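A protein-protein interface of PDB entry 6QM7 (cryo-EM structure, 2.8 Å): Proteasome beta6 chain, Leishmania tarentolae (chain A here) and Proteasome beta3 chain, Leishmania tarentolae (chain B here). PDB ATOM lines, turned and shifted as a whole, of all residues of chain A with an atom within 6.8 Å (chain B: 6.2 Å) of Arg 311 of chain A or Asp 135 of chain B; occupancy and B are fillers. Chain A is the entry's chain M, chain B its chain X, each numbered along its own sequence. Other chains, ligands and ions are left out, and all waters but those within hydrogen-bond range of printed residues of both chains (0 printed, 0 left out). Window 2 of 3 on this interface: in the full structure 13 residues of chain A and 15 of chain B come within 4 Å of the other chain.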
ATOM      1  N   PHE A 270      10.291   3.869   0.027  1.00  0.00           N
ATOM      2  CA  PHE A 270      10.072   2.411  -0.197  1.00  0.00           C
ATOM      3  C   PHE A 270      11.125   1.841  -1.140  1.00  0.00           C
ATOM      4  O   PHE A 270      11.614   0.709  -0.929  1.00  0.00           O
ATOM      5  CB  PHE A 270       8.779   2.068  -0.945  1.00  0.00           C
ATOM      6  CG  PHE A 270       7.504   2.481  -0.278  1.00  0.00           C
ATOM      7  CD1 PHE A 270       6.308   2.236  -0.913  1.00  0.00           C
ATOM      8  CD2 PHE A 270       7.489   3.140   0.945  1.00  0.00           C
ATOM      9  CE1 PHE A 270       5.114   2.632  -0.332  1.00  0.00           C
ATOM     10  CE2 PHE A 270       6.295   3.536   1.526  1.00  0.00           C
ATOM     11  CZ  PHE A 270       5.104   3.281   0.886  1.00  0.00           C
ATOM     12  N   PHE A 305       8.574  -0.526  -8.785  1.00  0.00           N
ATOM     13  CA  PHE A 305       7.402   0.349  -9.048  1.00  0.00           C
ATOM     14  C   PHE A 305       6.113  -0.397  -8.723  1.00  0.00           C
ATOM     15  O   PHE A 305       5.259   0.188  -8.042  1.00  0.00           O
ATOM     16  CB  PHE A 305       7.389   0.865 -10.484  1.00  0.00           C
ATOM     17  CG  PHE A 305       8.013   2.224 -10.550  1.00  0.00           C
ATOM     18  CD1 PHE A 305       9.365   2.367 -10.808  1.00  0.00           C
ATOM     19  CD2 PHE A 305       7.264   3.343 -10.223  1.00  0.00           C
ATOM     20  CE1 PHE A 305       9.941   3.622 -10.810  1.00  0.00           C
ATOM     21  CE2 PHE A 305       7.843   4.601 -10.211  1.00  0.00           C
ATOM     22  CZ  PHE A 305       9.178   4.735 -10.511  1.00  0.00           C
ATOM     23  N   THR A 306       5.986  -1.636  -9.196  1.00  0.00           N
ATOM     24  CA  THR A 306       4.845  -2.527  -8.876  1.00  0.00           C
ATOM     25  C   THR A 306       4.623  -2.539  -7.355  1.00  0.00           C
ATOM     26  O   THR A 306       3.472  -2.406  -6.932  1.00  0.00           O
ATOM     27  CB  THR A 306       5.047  -3.904  -9.513  1.00  0.00           C
ATOM     28  OG1 THR A 306       4.811  -3.753 -10.911  1.00  0.00           O
ATOM     29  CG2 THR A 306       4.094  -4.939  -8.974  1.00  0.00           C
ATOM     30  N   GLY A 307       5.687  -2.645  -6.570  1.00  0.00           N
ATOM     31  CA  GLY A 307       5.610  -2.620  -5.100  1.00  0.00           C
ATOM     32  C   GLY A 307       5.144  -1.268  -4.579  1.00  0.00           C
ATOM     33  O   GLY A 307       4.227  -1.235  -3.758  1.00  0.00           O
ATOM     34  N   ALA A 308       5.770  -0.188  -5.034  1.00  0.00           N
ATOM     35  CA  ALA A 308       5.438   1.201  -4.646  1.00  0.00           C
ATOM     36  C   ALA A 308       3.975   1.491  -4.968  1.00  0.00           C
ATOM     37  O   ALA A 308       3.319   2.087  -4.120  1.00  0.00           O
ATOM     38  CB  ALA A 308       6.339   2.184  -5.356  1.00  0.00           C
ATOM     39  N   ALA A 309       3.515   1.110  -6.161  1.00  0.00           N
ATOM     40  CA  ALA A 309       2.135   1.307  -6.658  1.00  0.00           C
ATOM     41  C   ALA A 309       1.133   0.633  -5.721  1.00  0.00           C
ATOM     42  O   ALA A 309       0.054   1.209  -5.501  1.00  0.00           O
ATOM     43  CB  ALA A 309       2.005   0.744  -8.053  1.00  0.00           C
ATOM     44  N   GLU A 310       1.482  -0.551  -5.223  1.00  0.00           N
ATOM     45  CA  GLU A 310       0.641  -1.382  -4.324  1.00  0.00           C
ATOM     46  C   GLU A 310       0.461  -0.684  -2.972  1.00  0.00           C
ATOM     47  O   GLU A 310      -0.659  -0.790  -2.422  1.00  0.00           O
ATOM     48  CB  GLU A 310       1.283  -2.751  -4.085  1.00  0.00           C
ATOM     49  CG  GLU A 310       0.334  -3.927  -4.258  1.00  0.00           C
ATOM     50  CD  GLU A 310       0.289  -4.574  -5.640  1.00  0.00           C
ATOM     51  OE1 GLU A 310       1.015  -4.120  -6.556  1.00  0.00           O
ATOM     52  OE2 GLU A 310      -0.494  -5.536  -5.801  1.00  0.00           O
ATOM     53  N   ARG A 311       1.503  -0.018  -2.462  1.00  0.00           N
ATOM     54  CA  ARG A 311       1.579   0.438  -1.049  1.00  0.00           C
ATOM     55  C   ARG A 311       1.507   1.961  -0.922  1.00  0.00           C
ATOM     56  O   ARG A 311       0.962   2.419   0.098  1.00  0.00           O
ATOM     57  CB  ARG A 311       2.862  -0.059  -0.384  1.00  0.00           C
ATOM     58  CG  ARG A 311       2.922  -1.568  -0.232  1.00  0.00           C
ATOM     59  CD  ARG A 311       1.994  -2.064   0.852  1.00  0.00           C
ATOM     60  NE  ARG A 311       1.992  -3.514   0.889  1.00  0.00           N
ATOM     61  CZ  ARG A 311       1.398  -4.244   1.813  1.00  0.00           C
ATOM     62  NH1 ARG A 311       0.752  -3.672   2.817  1.00  0.00           N
ATOM     63  NH2 ARG A 311       1.475  -5.561   1.739  1.00  0.00           N
ATOM     64  N   ASP A 312       2.077   2.717  -1.860  1.00  0.00           N
ATOM     65  CA  ASP A 312       1.966   4.201  -1.892  1.00  0.00           C
ATOM     66  C   ASP A 312       0.663   4.557  -2.597  1.00  0.00           C
ATOM     67  O   ASP A 312       0.397   4.012  -3.693  1.00  0.00           O
ATOM     68  CB  ASP A 312       3.154   4.868  -2.583  1.00  0.00           C
ATOM     69  CG  ASP A 312       3.134   6.393  -2.526  1.00  0.00           C
ATOM     70  OD1 ASP A 312       2.696   6.960  -1.484  1.00  0.00           O
ATOM     71  OD2 ASP A 312       3.564   7.012  -3.532  1.00  0.00           O
ATOM     72  N   ILE A 313      -0.125   5.432  -1.985  1.00  0.00           N
ATOM     73  CA  ILE A 313      -1.483   5.767  -2.491  1.00  0.00           C
ATOM     74  C   ILE A 313      -1.360   6.812  -3.599  1.00  0.00           C
ATOM     75  O   ILE A 313      -2.353   6.988  -4.314  1.00  0.00           O
ATOM     76  CB  ILE A 313      -2.416   6.216  -1.352  1.00  0.00           C
ATOM     77  CG1 ILE A 313      -1.946   7.515  -0.690  1.00  0.00           C
ATOM     78  CG2 ILE A 313      -2.611   5.093  -0.339  1.00  0.00           C
ATOM     79  CD1 ILE A 313      -2.933   8.070   0.318  1.00  0.00           C
ATOM     80  N   TYR A 314      -0.208   7.472  -3.730  1.00  0.00           N
ATOM     81  CA  TYR A 314       0.031   8.572  -4.694  1.00  0.00           C
ATOM     82  C   TYR A 314       0.895   8.123  -5.875  1.00  0.00           C
ATOM     83  O   TYR A 314       1.129   8.943  -6.771  1.00  0.00           O
ATOM     84  CB  TYR A 314       0.660   9.760  -3.966  1.00  0.00           C
ATOM     85  CG  TYR A 314      -0.226  10.368  -2.911  1.00  0.00           C
ATOM     86  CD1 TYR A 314      -1.533  10.732  -3.204  1.00  0.00           C
ATOM     87  CD2 TYR A 314       0.234  10.582  -1.619  1.00  0.00           C
ATOM     88  CE1 TYR A 314      -2.366  11.288  -2.245  1.00  0.00           C
ATOM     89  CE2 TYR A 314      -0.589  11.132  -0.646  1.00  0.00           C
ATOM     90  CZ  TYR A 314      -1.891  11.489  -0.961  1.00  0.00           C
ATOM     91  OH  TYR A 314      -2.715  12.031  -0.017  1.00  0.00           O
ATOM     92  N   THR A 315       1.368   6.883  -5.893  1.00  0.00           N
ATOM     93  CA  THR A 315       2.079   6.288  -7.052  1.00  0.00           C
ATOM     94  C   THR A 315       1.124   5.291  -7.697  1.00  0.00           C
ATOM     95  O   THR A 315       0.409   4.581  -6.932  1.00  0.00           O
ATOM     96  CB  THR A 315       3.405   5.646  -6.625  1.00  0.00           C
ATOM     97  OG1 THR A 315       4.203   6.672  -6.035  1.00  0.00           O
ATOM     98  CG2 THR A 315       4.162   4.999  -7.768  1.00  0.00           C
ATOM     99  N   ARG A 337      -1.122  -0.937 -10.932  1.00  0.00           N
ATOM    100  CA  ARG A 337      -2.468  -0.871 -10.307  1.00  0.00           C
ATOM    101  C   ARG A 337      -3.091   0.483 -10.643  1.00  0.00           C
ATOM    102  O   ARG A 337      -2.482   1.517 -10.299  1.00  0.00           O
ATOM    103  CB  ARG A 337      -2.402  -1.052  -8.785  1.00  0.00           C
ATOM    104  CG  ARG A 337      -3.011  -2.356  -8.295  1.00  0.00           C
ATOM    105  CD  ARG A 337      -2.357  -2.833  -7.021  1.00  0.00           C
ATOM    106  NE  ARG A 337      -3.162  -3.799  -6.282  1.00  0.00           N
ATOM    107  CZ  ARG A 337      -4.108  -3.508  -5.384  1.00  0.00           C
ATOM    108  NH1 ARG A 337      -4.746  -4.494  -4.771  1.00  0.00           N
ATOM    109  NH2 ARG A 337      -4.421  -2.251  -5.095  1.00  0.00           N
ATOM    110  N   ALA B  13       6.815  -7.914  11.641  1.00  0.00           N
ATOM    111  CA  ALA B  13       6.423  -9.333  11.709  1.00  0.00           C
ATOM    112  C   ALA B  13       5.959  -9.767  10.325  1.00  0.00           C
ATOM    113  O   ALA B  13       5.449  -8.939   9.587  1.00  0.00           O
ATOM    114  CB  ALA B  13       5.361  -9.548  12.757  1.00  0.00           C
ATOM    115  N   MET B  14       6.094 -11.053  10.047  1.00  0.00           N
ATOM    116  CA  MET B  14       5.979 -11.628   8.696  1.00  0.00           C
ATOM    117  C   MET B  14       5.441 -13.033   8.797  1.00  0.00           C
ATOM    118  O   MET B  14       5.983 -13.788   9.605  1.00  0.00           O
ATOM    119  CB  MET B  14       7.357 -11.701   8.057  1.00  0.00           C
ATOM    120  CG  MET B  14       7.468 -10.754   6.942  1.00  0.00           C
ATOM    121  SD  MET B  14       9.074 -10.787   6.225  1.00  0.00           S
ATOM    122  CE  MET B  14       8.930  -9.318   5.200  1.00  0.00           C
ATOM    123  N   ALA B  15       4.454 -13.364   7.973  1.00  0.00           N
ATOM    124  CA  ALA B  15       3.750 -14.659   8.007  1.00  0.00           C
ATOM    125  C   ALA B  15       4.350 -15.560   6.944  1.00  0.00           C
ATOM    126  O   ALA B  15       4.436 -15.133   5.800  1.00  0.00           O
ATOM    127  CB  ALA B  15       2.285 -14.445   7.769  1.00  0.00           C
ATOM    128  N   GLY B  16       4.746 -16.765   7.325  1.00  0.00           N
ATOM    129  CA  GLY B  16       5.134 -17.825   6.378  1.00  0.00           C
ATOM    130  C   GLY B  16       4.146 -18.965   6.440  1.00  0.00           C
ATOM    131  O   GLY B  16       3.054 -18.778   7.001  1.00  0.00           O
ATOM    132  N   LEU B 121      -0.985 -12.197  12.332  1.00  0.00           N
ATOM    133  CA  LEU B 121      -0.286 -10.924  12.600  1.00  0.00           C
ATOM    134  C   LEU B 121      -1.326  -9.873  12.914  1.00  0.00           C
ATOM    135  O   LEU B 121      -2.392  -9.922  12.300  1.00  0.00           O
ATOM    136  CB  LEU B 121       0.488 -10.480  11.366  1.00  0.00           C
ATOM    137  CG  LEU B 121       1.372 -11.540  10.741  1.00  0.00           C
ATOM    138  CD1 LEU B 121       1.966 -10.987   9.459  1.00  0.00           C
ATOM    139  CD2 LEU B 121       2.440 -11.989  11.723  1.00  0.00           C
ATOM    140  N   PRO B 133      -3.240  -8.163   8.433  1.00  0.00           N
ATOM    141  CA  PRO B 133      -3.009  -8.664   7.086  1.00  0.00           C
ATOM    142  C   PRO B 133      -2.410 -10.069   7.027  1.00  0.00           C
ATOM    143  O   PRO B 133      -1.832 -10.505   7.994  1.00  0.00           O
ATOM    144  CB  PRO B 133      -1.991  -7.666   6.546  1.00  0.00           C
ATOM    145  CG  PRO B 133      -1.161  -7.348   7.757  1.00  0.00           C
ATOM    146  CD  PRO B 133      -2.155  -7.300   8.896  1.00  0.00           C
ATOM    147  N   GLU B 134      -2.558 -10.701   5.864  1.00  0.00           N
ATOM    148  CA  GLU B 134      -2.073 -12.066   5.533  1.00  0.00           C
ATOM    149  C   GLU B 134      -0.540 -12.113   5.544  1.00  0.00           C
ATOM    150  O   GLU B 134      -0.014 -13.208   5.796  1.00  0.00           O
ATOM    151  CB  GLU B 134      -2.586 -12.512   4.153  1.00  0.00           C
ATOM    152  CG  GLU B 134      -2.397 -11.470   3.036  1.00  0.00           C
ATOM    153  CD  GLU B 134      -1.983 -11.982   1.659  1.00  0.00           C
ATOM    154  OE1 GLU B 134      -1.268 -11.236   0.943  1.00  0.00           O
ATOM    155  OE2 GLU B 134      -2.371 -13.119   1.299  1.00  0.00           O
ATOM    156  N   ASP B 135       0.138 -10.996   5.241  1.00  0.00           N
ATOM    157  CA  ASP B 135       1.550 -10.997   4.763  1.00  0.00           C
ATOM    158  C   ASP B 135       2.520 -10.584   5.869  1.00  0.00           C
ATOM    159  O   ASP B 135       3.305 -11.422   6.318  1.00  0.00           O
ATOM    160  CB  ASP B 135       1.755 -10.152   3.495  1.00  0.00           C
ATOM    161  CG  ASP B 135       1.136  -8.764   3.432  1.00  0.00           C
ATOM    162  OD1 ASP B 135       0.800  -8.199   4.497  1.00  0.00           O
ATOM    163  OD2 ASP B 135       0.991  -8.259   2.293  1.00  0.00           O
ATOM    164  N   TYR B 136       2.479  -9.327   6.268  1.00  0.00           N
ATOM    165  CA  TYR B 136       3.478  -8.721   7.167  1.00  0.00           C
ATOM    166  C   TYR B 136       2.901  -7.453   7.785  1.00  0.00           C
ATOM    167  O   TYR B 136       2.018  -6.811   7.207  1.00  0.00           O
ATOM    168  CB  TYR B 136       4.742  -8.422   6.370  1.00  0.00           C
ATOM    169  CG  TYR B 136       4.597  -7.259   5.432  1.00  0.00           C
ATOM    170  CD1 TYR B 136       4.680  -5.965   5.912  1.00  0.00           C
ATOM    171  CD2 TYR B 136       4.369  -7.445   4.077  1.00  0.00           C
ATOM    172  CE1 TYR B 136       4.537  -4.875   5.074  1.00  0.00           C
ATOM    173  CE2 TYR B 136       4.232  -6.366   3.221  1.00  0.00           C
ATOM    174  CZ  TYR B 136       4.312  -5.073   3.722  1.00  0.00           C
ATOM    175  OH  TYR B 136       4.185  -3.972   2.917  1.00  0.00           O
ATOM    176  N   VAL B 137       3.402  -7.096   8.948  1.00  0.00           N
ATOM    177  CA  VAL B 137       3.048  -5.828   9.625  1.00  0.00           C
ATOM    178  C   VAL B 137       4.354  -5.230  10.079  1.00  0.00           C
ATOM    179  O   VAL B 137       5.271  -5.999  10.332  1.00  0.00           O
ATOM    180  CB  VAL B 137       2.115  -6.050  10.825  1.00  0.00           C
ATOM    181  CG1 VAL B 137       0.736  -6.499  10.377  1.00  0.00           C
ATOM    182  CG2 VAL B 137       2.691  -7.027  11.844  1.00  0.00           C
ATOM    183  N   HIS B 147       7.854  -1.352   4.930  1.00  0.00           N
ATOM    184  CA  HIS B 147       6.734  -1.585   3.977  1.00  0.00           C
ATOM    185  C   HIS B 147       7.281  -1.803   2.563  1.00  0.00           C
ATOM    186  O   HIS B 147       6.776  -2.695   1.882  1.00  0.00           O
ATOM    187  CB  HIS B 147       5.740  -0.416   3.989  1.00  0.00           C
ATOM    188  CG  HIS B 147       4.715  -0.528   5.061  1.00  0.00           C
ATOM    189  ND1 HIS B 147       4.589   0.410   6.072  1.00  0.00           N
ATOM    190  CD2 HIS B 147       3.772  -1.466   5.286  1.00  0.00           C
ATOM    191  CE1 HIS B 147       3.605   0.055   6.871  1.00  0.00           C
ATOM    192  NE2 HIS B 147       3.091  -1.096   6.415  1.00  0.00           N
ATOM    193  N   GLY B 148       8.254  -0.999   2.136  1.00  0.00           N
ATOM    194  CA  GLY B 148       8.840  -1.104   0.792  1.00  0.00           C
ATOM    195  C   GLY B 148       9.592  -2.406   0.621  1.00  0.00           C
ATOM    196  O   GLY B 148       9.433  -3.056  -0.432  1.00  0.00           O
ATOM    197  N   GLU B 151       7.106  -5.547   1.037  1.00  0.00           N
ATOM    198  CA  GLU B 151       6.249  -5.633  -0.178  1.00  0.00           C
ATOM    199  C   GLU B 151       7.003  -6.347  -1.302  1.00  0.00           C
ATOM    200  O   GLU B 151       6.378  -7.177  -2.021  1.00  0.00           O
ATOM    201  CB  GLU B 151       5.836  -4.238  -0.665  1.00  0.00           C
ATOM    202  CG  GLU B 151       5.030  -4.216  -1.968  1.00  0.00           C
ATOM    203  CD  GLU B 151       3.729  -5.014  -2.003  1.00  0.00           C
ATOM    204  OE1 GLU B 151       3.308  -5.420  -3.117  1.00  0.00           O
ATOM    205  OE2 GLU B 151       3.128  -5.227  -0.916  1.00  0.00           O
ATOM    206  N   TRP B 154       8.649 -10.263   0.184  1.00  0.00           N
ATOM    207  CA  TRP B 154       7.718 -11.232   0.807  1.00  0.00           C
ATOM    208  C   TRP B 154       6.903 -11.953  -0.268  1.00  0.00           C
ATOM    209  O   TRP B 154       6.377 -11.258  -1.163  1.00  0.00           O
ATOM    210  CB  TRP B 154       6.800 -10.531   1.806  1.00  0.00           C
ATOM    211  CG  TRP B 154       5.948 -11.498   2.556  1.00  0.00           C
ATOM    212  CD1 TRP B 154       6.273 -12.160   3.701  1.00  0.00           C
ATOM    213  CD2 TRP B 154       4.647 -11.958   2.167  1.00  0.00           C
ATOM    214  NE1 TRP B 154       5.252 -12.993   4.062  1.00  0.00           N
ATOM    215  CE2 TRP B 154       4.238 -12.885   3.149  1.00  0.00           C
ATOM    216  CE3 TRP B 154       3.793 -11.670   1.095  1.00  0.00           C
ATOM    217  CZ2 TRP B 154       3.005 -13.532   3.083  1.00  0.00           C
ATOM    218  CZ3 TRP B 154       2.574 -12.309   1.027  1.00  0.00           C
ATOM    219  CH2 TRP B 154       2.184 -13.220   2.018  1.00  0.00           C
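Of the 14 printed residues of chain B, 4 touch a printed residue of chain A. Printed residues of chain B that touch a printed residue of chain A: Asp 135, Tyr 136, Gly 148 and Glu 151. Hydrophobic or aromatic side chains of chain B within 4 Å of the printed part of chain A: Tyr 136. Hydrophobic or aromatic side chains of chain A within 4 Å of the printed part of chain B: Phe 270. Along chain A the printed residues that touch a printed residue of chain B span positions 270 to 311. Among the printed residues, Asp or Glu carboxylates within 4 Å of a Lys or Arg side-chain nitrogen of the other chain: Arg 311 of chain A with Asp 135 of chain B (2.8 Å) and Arg 311 of chain A with Glu 151 of chain B (2.7 Å).
The side-chain carboxylate (OD2) of Asp 135 of chain B is in salt-bridge range of the guanidinium group (NH2) of Arg 311 of chain A, 2.8 Å away. The side-chain hydroxyl (OH) of Tyr 136 of chain B lies close to the guanidinium group (NE) of Arg 311 of chain A, at 3.0 Å. NE of Arg 311 of chain A lies within salt-bridge range of OE2 of Glu 151 of chain B (2.7 Å).
Among the printed residues, pairs that only touch across the chains: Glu 310 of chain A with Glu 151 of chain B, Gly 307 of chain A with Glu 151 of chain B and Phe 270 of chain A with Gly 148 of chain B.
N of Ala 15 of chain B sits at hydrogen-bond distance from O of Asp 135 of chain B (2.8 Å). O of Asp 135 of chain B sits at hydrogen-bond distance from NE1 of Trp 154 of chain B (3.4 Å). The backbone carbonyl oxygen (O) of His 147 of chain B is in hydrogen-bond range of the side-chain hydroxyl (OH) of Tyr 136 of chain B, at 3.1 Å. OE2 of Glu 310 of chain A lies within salt-bridge range of NE of Arg 337 of chain A (3.2 Å).
Of the printed residues of chain B, Phe 270 of chain A touches Gly 148 (3.6 Å). Of the printed residues of chain B, Gly 307 of chain A touches Glu 151 (3.6 Å). Printed residues of chain B within 4 Å of Glu 310 of chain A: Glu 151 (3.5 Å). Of the printed residues of chain B, Arg 311 of chain A touches Asp 135 (2.8 Å), Tyr 136 (3.0 Å) and Glu 151 (2.7 Å). Asp 135 of chain B touches just one residue of chain A: Arg 311. Of the printed residues of chain A, Tyr 136 of chain B touches Arg 311. Of the printed residues of chain A, Gly 148 of chain B touches Phe 270.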
